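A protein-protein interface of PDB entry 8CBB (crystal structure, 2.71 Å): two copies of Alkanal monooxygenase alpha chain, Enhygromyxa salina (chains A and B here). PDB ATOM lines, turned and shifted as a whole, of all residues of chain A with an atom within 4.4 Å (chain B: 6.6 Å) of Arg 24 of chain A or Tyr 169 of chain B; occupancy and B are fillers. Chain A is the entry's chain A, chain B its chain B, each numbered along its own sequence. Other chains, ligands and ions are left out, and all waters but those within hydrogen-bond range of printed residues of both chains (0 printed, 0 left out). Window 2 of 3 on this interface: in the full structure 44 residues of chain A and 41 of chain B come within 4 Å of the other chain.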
ATOM      1  N   THR A  22       2.478   5.825   9.081  1.00  0.00           N
ATOM      2  CA  THR A  22       3.738   6.295   8.531  1.00  0.00           C
ATOM      3  C   THR A  22       4.713   6.570   9.674  1.00  0.00           C
ATOM      4  O   THR A  22       4.300   6.778  10.813  1.00  0.00           O
ATOM      5  CB  THR A  22       3.524   7.539   7.658  1.00  0.00           C
ATOM      6  OG1 THR A  22       2.999   8.581   8.481  1.00  0.00           O
ATOM      7  CG2 THR A  22       2.586   7.287   6.498  1.00  0.00           C
ATOM      8  N   GLU A  23       6.011   6.563   9.352  1.00  0.00           N
ATOM      9  CA  GLU A  23       7.047   6.900  10.314  1.00  0.00           C
ATOM     10  C   GLU A  23       6.818   8.320  10.824  1.00  0.00           C
ATOM     11  O   GLU A  23       6.974   8.591  12.013  1.00  0.00           O
ATOM     12  CB  GLU A  23       8.433   6.765   9.678  1.00  0.00           C
ATOM     13  CG  GLU A  23       8.814   5.333   9.342  1.00  0.00           C
ATOM     14  CD  GLU A  23      10.255   5.146   8.897  1.00  0.00           C
ATOM     15  OE1 GLU A  23      10.726   3.990   8.886  1.00  0.00           O
ATOM     16  OE2 GLU A  23      10.903   6.157   8.565  1.00  0.00           O
ATOM     17  N   ARG A  24       6.447   9.219   9.908  1.00  0.00           N
ATOM     18  CA  ARG A  24       6.292  10.627  10.227  1.00  0.00           C
ATOM     19  C   ARG A  24       5.185  10.784  11.267  1.00  0.00           C
ATOM     20  O   ARG A  24       5.341  11.524  12.235  1.00  0.00           O
ATOM     21  CB  ARG A  24       5.985  11.429   8.957  1.00  0.00           C
ATOM     22  CG  ARG A  24       5.416  12.817   9.213  1.00  0.00           C
ATOM     23  CD  ARG A  24       6.425  13.923   8.965  1.00  0.00           C
ATOM     24  NE  ARG A  24       7.368  14.066  10.067  1.00  0.00           N
ATOM     25  CZ  ARG A  24       7.858  15.225  10.494  1.00  0.00           C
ATOM     26  NH1 ARG A  24       7.247  16.357  10.192  1.00  0.00           N
ATOM     27  NH2 ARG A  24       8.959  15.245  11.225  1.00  0.00           N
ATOM     28  N   ARG A  25       4.071  10.074  11.051  1.00  0.00           N
ATOM     29  CA  ARG A  25       2.893  10.209  11.891  1.00  0.00           C
ATOM     30  C   ARG A  25       3.225   9.749  13.308  1.00  0.00           C
ATOM     31  O   ARG A  25       2.867  10.408  14.282  1.00  0.00           O
ATOM     32  CB  ARG A  25       1.732   9.387  11.320  1.00  0.00           C
ATOM     33  CG  ARG A  25       0.444   9.490  12.123  1.00  0.00           C
ATOM     34  CD  ARG A  25      -0.193  10.868  12.017  1.00  0.00           C
ATOM     35  NE  ARG A  25      -1.478  10.936  12.698  1.00  0.00           N
ATOM     36  CZ  ARG A  25      -2.078  12.069  13.061  1.00  0.00           C
ATOM     37  NH1 ARG A  25      -1.493  13.235  12.835  1.00  0.00           N
ATOM     38  NH2 ARG A  25      -3.262  12.030  13.647  1.00  0.00           N
ATOM     39  N   VAL A  26       3.914   8.607  13.398  1.00  0.00           N
ATOM     40  CA  VAL A  26       4.286   8.021  14.674  1.00  0.00           C
ATOM     41  C   VAL A  26       5.136   9.024  15.452  1.00  0.00           C
ATOM     42  O   VAL A  26       4.895   9.264  16.632  1.00  0.00           O
ATOM     43  CB  VAL A  26       5.026   6.684  14.475  1.00  0.00           C
ATOM     44  CG1 VAL A  26       5.708   6.218  15.752  1.00  0.00           C
ATOM     45  CG2 VAL A  26       4.101   5.604  13.934  1.00  0.00           C
ATOM     46  N   LEU A  27       6.130   9.607  14.773  1.00  0.00           N
ATOM     47  CA  LEU A  27       7.126  10.440  15.426  1.00  0.00           C
ATOM     48  C   LEU A  27       6.514  11.791  15.791  1.00  0.00           C
ATOM     49  O   LEU A  27       7.014  12.480  16.677  1.00  0.00           O
ATOM     50  CB  LEU A  27       8.326  10.608  14.489  1.00  0.00           C
ATOM     51  CG  LEU A  27       9.224   9.378  14.349  1.00  0.00           C
ATOM     52  CD1 LEU A  27      10.271   9.585  13.266  1.00  0.00           C
ATOM     53  CD2 LEU A  27       9.888   9.039  15.675  1.00  0.00           C
ATOM     54  N   GLU A  28       5.430  12.157  15.099  1.00  0.00           N
ATOM     55  CA  GLU A  28       4.759  13.427  15.326  1.00  0.00           C
ATOM     56  C   GLU A  28       3.763  13.272  16.473  1.00  0.00           C
ATOM     57  O   GLU A  28       3.633  14.162  17.311  1.00  0.00           O
ATOM     58  CB  GLU A  28       4.058  13.893  14.049  1.00  0.00           C
ATOM     59  CG  GLU A  28       4.997  14.523  13.033  1.00  0.00           C
ATOM     60  CD  GLU A  28       5.036  16.041  13.061  1.00  0.00           C
ATOM     61  OE1 GLU A  28       4.077  16.667  12.560  1.00  0.00           O
ATOM     62  OE2 GLU A  28       6.023  16.596  13.584  1.00  0.00           O
ATOM     63  N   ALA B  97      18.903  10.875  11.537  1.00  0.00           N
ATOM     64  CA  ALA B  97      17.658  10.705  10.807  1.00  0.00           C
ATOM     65  C   ALA B  97      16.475  10.915  11.749  1.00  0.00           C
ATOM     66  O   ALA B  97      15.429  11.412  11.338  1.00  0.00           O
ATOM     67  CB  ALA B  97      17.620   9.340  10.163  1.00  0.00           C
ATOM     68  N   ASP B 100      16.363  14.662  12.459  1.00  0.00           N
ATOM     69  CA  ASP B 100      15.829  15.298  11.267  1.00  0.00           C
ATOM     70  C   ASP B 100      14.306  15.226  11.303  1.00  0.00           C
ATOM     71  O   ASP B 100      13.625  16.179  10.931  1.00  0.00           O
ATOM     72  CB  ASP B 100      16.386  14.642  10.000  1.00  0.00           C
ATOM     73  CG  ASP B 100      15.856  15.239   8.709  1.00  0.00           C
ATOM     74  OD1 ASP B 100      16.112  16.436   8.466  1.00  0.00           O
ATOM     75  OD2 ASP B 100      15.197  14.500   7.952  1.00  0.00           O
ATOM     76  N   GLN B 101      13.787  14.079  11.755  1.00  0.00           N
ATOM     77  CA  GLN B 101      12.354  13.868  11.861  1.00  0.00           C
ATOM     78  C   GLN B 101      11.800  14.721  12.999  1.00  0.00           C
ATOM     79  O   GLN B 101      10.827  15.448  12.817  1.00  0.00           O
ATOM     80  CB  GLN B 101      12.048  12.384  12.079  1.00  0.00           C
ATOM     81  CG  GLN B 101      12.148  11.546  10.812  1.00  0.00           C
ATOM     82  CD  GLN B 101      10.860  11.516  10.025  1.00  0.00           C
ATOM     83  OE1 GLN B 101       9.849  12.092  10.423  1.00  0.00           O
ATOM     84  NE2 GLN B 101      10.888  10.835   8.891  1.00  0.00           N
ATOM     85  N   LEU B 102      12.434  14.625  14.173  1.00  0.00           N
ATOM     86  CA  LEU B 102      11.981  15.346  15.351  1.00  0.00           C
ATOM     87  C   LEU B 102      11.995  16.846  15.071  1.00  0.00           C
ATOM     88  O   LEU B 102      11.077  17.564  15.465  1.00  0.00           O
ATOM     89  CB  LEU B 102      12.890  14.997  16.534  1.00  0.00           C
ATOM     90  CG  LEU B 102      12.758  13.573  17.072  1.00  0.00           C
ATOM     91  CD1 LEU B 102      13.703  13.346  18.243  1.00  0.00           C
ATOM     92  CD2 LEU B 102      11.323  13.275  17.480  1.00  0.00           C
ATOM     93  N   SER B 103      13.049  17.307  14.387  1.00  0.00           N
ATOM     94  CA  SER B 103      13.331  18.727  14.266  1.00  0.00           C
ATOM     95  C   SER B 103      12.646  19.294  13.027  1.00  0.00           C
ATOM     96  O   SER B 103      12.763  20.484  12.739  1.00  0.00           O
ATOM     97  CB  SER B 103      14.813  18.981  14.227  1.00  0.00           C
ATOM     98  OG  SER B 103      15.370  18.534  12.999  1.00  0.00           O
ATOM     99  N   ASP B 104      11.938  18.427  12.296  1.00  0.00           N
ATOM    100  CA  ASP B 104      11.238  18.826  11.087  1.00  0.00           C
ATOM    101  C   ASP B 104      12.248  19.387  10.088  1.00  0.00           C
ATOM    102  O   ASP B 104      11.949  20.323   9.348  1.00  0.00           O
ATOM    103  CB  ASP B 104      10.128  19.836  11.401  1.00  0.00           C
ATOM    104  CG  ASP B 104       9.104  19.327  12.403  1.00  0.00           C
ATOM    105  OD1 ASP B 104       8.337  18.410  12.044  1.00  0.00           O
ATOM    106  OD2 ASP B 104       9.082  19.852  13.533  1.00  0.00           O
ATOM    107  N   GLY B 105      13.449  18.797  10.083  1.00  0.00           N
ATOM    108  CA  GLY B 105      14.445  19.084   9.064  1.00  0.00           C
ATOM    109  C   GLY B 105      15.186  20.389   9.338  1.00  0.00           C
ATOM    110  O   GLY B 105      15.542  21.109   8.407  1.00  0.00           O
ATOM    111  N   ARG B 106      15.417  20.675  10.624  1.00  0.00           N
ATOM    112  CA  ARG B 106      16.072  21.906  11.041  1.00  0.00           C
ATOM    113  C   ARG B 106      17.518  21.609  11.434  1.00  0.00           C
ATOM    114  O   ARG B 106      18.199  22.467  11.994  1.00  0.00           O
ATOM    115  CB  ARG B 106      15.323  22.538  12.218  1.00  0.00           C
ATOM    116  CG  ARG B 106      14.114  23.373  11.820  1.00  0.00           C
ATOM    117  CD  ARG B 106      13.599  24.219  12.969  1.00  0.00           C
ATOM    118  NE  ARG B 106      13.159  23.410  14.099  1.00  0.00           N
ATOM    119  CZ  ARG B 106      13.542  23.593  15.359  1.00  0.00           C
ATOM    120  NH1 ARG B 106      14.478  24.479  15.649  1.00  0.00           N
ATOM    121  NH2 ARG B 106      12.986  22.886  16.328  1.00  0.00           N
ATOM    122  N   ARG B 167      13.655   6.765   8.303  1.00  0.00           N
ATOM    123  CA  ARG B 167      14.075   7.554   7.157  1.00  0.00           C
ATOM    124  C   ARG B 167      14.088   9.032   7.539  1.00  0.00           C
ATOM    125  O   ARG B 167      13.269   9.479   8.342  1.00  0.00           O
ATOM    126  CB  ARG B 167      13.139   7.320   5.966  1.00  0.00           C
ATOM    127  CG  ARG B 167      13.046   5.867   5.523  1.00  0.00           C
ATOM    128  CD  ARG B 167      14.342   5.367   4.917  1.00  0.00           C
ATOM    129  NE  ARG B 167      14.701   6.106   3.715  1.00  0.00           N
ATOM    130  CZ  ARG B 167      14.488   5.674   2.477  1.00  0.00           C
ATOM    131  NH1 ARG B 167      13.892   4.513   2.273  1.00  0.00           N
ATOM    132  NH2 ARG B 167      14.873   6.407   1.445  1.00  0.00           N
ATOM    133  N   PRO B 168      15.015   9.834   6.973  1.00  0.00           N
ATOM    134  CA  PRO B 168      14.959  11.289   7.103  1.00  0.00           C
ATOM    135  C   PRO B 168      13.584  11.853   6.758  1.00  0.00           C
ATOM    136  O   PRO B 168      12.850  11.272   5.961  1.00  0.00           O
ATOM    137  CB  PRO B 168      16.023  11.773   6.107  1.00  0.00           C
ATOM    138  CG  PRO B 168      17.016  10.632   6.046  1.00  0.00           C
ATOM    139  CD  PRO B 168      16.171   9.381   6.185  1.00  0.00           C
ATOM    140  N   TYR B 169      13.251  12.988   7.381  1.00  0.00           N
ATOM    141  CA  TYR B 169      12.158  13.837   6.937  1.00  0.00           C
ATOM    142  C   TYR B 169      12.548  14.528   5.632  1.00  0.00           C
ATOM    143  O   TYR B 169      11.727  14.662   4.727  1.00  0.00           O
ATOM    144  CB  TYR B 169      11.815  14.851   8.032  1.00  0.00           C
ATOM    145  CG  TYR B 169      10.771  15.874   7.662  1.00  0.00           C
ATOM    146  CD1 TYR B 169       9.499  15.491   7.269  1.00  0.00           C
ATOM    147  CD2 TYR B 169      11.050  17.229   7.721  1.00  0.00           C
ATOM    148  CE1 TYR B 169       8.534  16.427   6.937  1.00  0.00           C
ATOM    149  CE2 TYR B 169      10.096  18.178   7.392  1.00  0.00           C
ATOM    150  CZ  TYR B 169       8.833  17.776   6.998  1.00  0.00           C
ATOM    151  OH  TYR B 169       7.884  18.711   6.668  1.00  0.00           O
ATOM    152  N   SER B 170      13.813  14.959   5.557  1.00  0.00           N
ATOM    153  CA  SER B 170      14.324  15.682   4.404  1.00  0.00           C
ATOM    154  C   SER B 170      14.577  14.711   3.253  1.00  0.00           C
ATOM    155  O   SER B 170      14.923  13.553   3.477  1.00  0.00           O
ATOM    156  CB  SER B 170      15.578  16.441   4.756  1.00  0.00           C
ATOM    157  OG  SER B 170      15.441  17.100   6.006  1.00  0.00           O
ATOM    158  N   ASP B 171      14.405  15.204   2.021  1.00  0.00           N
ATOM    159  CA  ASP B 171      14.767  14.453   0.832  1.00  0.00           C
ATOM    160  C   ASP B 171      16.233  14.041   0.935  1.00  0.00           C
ATOM    161  O   ASP B 171      16.567  12.870   0.771  1.00  0.00           O
ATOM    162  CB  ASP B 171      14.510  15.269  -0.438  1.00  0.00           C
ATOM    163  CG  ASP B 171      13.040  15.562  -0.688  1.00  0.00           C
ATOM    164  OD1 ASP B 171      12.242  14.602  -0.667  1.00  0.00           O
ATOM    165  OD2 ASP B 171      12.705  16.744  -0.902  1.00  0.00           O
ATOM    166  N   LYS B 172      17.092  15.026   1.211  1.00  0.00           N
ATOM    167  CA  LYS B 172      18.501  14.785   1.470  1.00  0.00           C
ATOM    168  C   LYS B 172      18.845  15.303   2.864  1.00  0.00           C
ATOM    169  O   LYS B 172      18.471  16.416   3.228  1.00  0.00           O
ATOM    170  CB  LYS B 172      19.360  15.469   0.401  1.00  0.00           C
ATOM    171  CG  LYS B 172      20.650  14.740   0.040  1.00  0.00           C
ATOM    172  N   MET B 173      19.558  14.477   3.637  1.00  0.00           N
ATOM    173  CA  MET B 173      20.054  14.876   4.944  1.00  0.00           C
ATOM    174  C   MET B 173      20.963  16.092   4.784  1.00  0.00           C
ATOM    175  O   MET B 173      22.003  16.011   4.134  1.00  0.00           O
ATOM    176  CB  MET B 173      20.835  13.737   5.603  1.00  0.00           C
ATOM    177  CG  MET B 173      21.493  14.126   6.914  1.00  0.00           C
ATOM    178  SD  MET B 173      20.288  14.509   8.210  1.00  0.00           S
ATOM    179  CE  MET B 173      19.447  12.933   8.349  1.00  0.00           C
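Of the 15 printed residues of chain B, 4 touch a printed residue of chain A. Printed residues of chain B that touch a printed residue of chain A: Gln 101, Asp 104, Arg 167 and Tyr 169. Hydrophobic or aromatic side chains of chain B that line the printed part of chain A: Tyr 169. Printed residues of chain A that touch a printed residue of chain B: Glu 23, Arg 24, Leu 27 and Glu 28. Among the printed residues, Asp or Glu carboxylates within 4 Å of a Lys or Arg side-chain nitrogen of the other chain: Arg 24 of chain A with Asp 104 of chain B (3.0 Å).
Of chain B, only Gln 101, Asp 104 and Tyr 169 come within 4 Å of Arg 24 of chain A. Of the printed residues of chain A, Gln 101 of chain B touches Arg 24 (2.5 Å) and Leu 27 (3.5 Å). Of the printed residues of chain B, Leu 27 of chain A touches Gln 101. Gly 105 of chain B touches none of the printed residues of chain A. Pro 168 of chain B touches none of the printed residues of chain A. The nearest residue of chain B that does not touch Arg 24 of chain A is Leu 102 of chain B (4.6 Å). The nearest printed residue of chain A that does not touch Tyr 169 of chain B is Glu 28 of chain A (7.1 Å).
The backbone carbonyl oxygen (O) of Arg 167 of chain B is in hydrogen-bond range of the side-chain amide nitrogen (NE2) of Gln 101 of chain B, 2.8 Å away. The guanidinium group (NH1) of Arg 24 of chain A is in salt-bridge range of the side-chain carboxylate (OE2) of Glu 28 of chain A (3.6 Å). OD2 of Asp 100 of chain B sits at hydrogen-bond distance from N of Tyr 169 of chain B (2.5 Å).
The guanidinium group of Arg 24 of chain A lies within salt-bridge range of the side-chain carboxylate of Asp 104 of chain B, 3.0 Å away. The backbone carbonyl oxygen (O) of Gln 101 of chain B sits at hydrogen-bond distance from the guanidinium group (NH2) of Arg 24 of chain A (2.5 Å). The backbone NH of Arg 167 of chain B lies within hydrogen-bond range of the side-chain carboxylate of Glu 23 of chain A. OD1 of Asp 104 of chain B lies close to OE2 of Glu 28 of chain A (3.3 Å).
Among the printed residues, pairs that only touch across the chains: Arg 24 of chain A with Tyr 169 of chain B (3.5 Å) and Leu 27 of chain A with Gln 101 of chain B (3.5 Å).
No position is printed for both chains. Of the 6 pairs that touch across the chains among the printed residues, none has its exchanged pair printed and touching as well.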
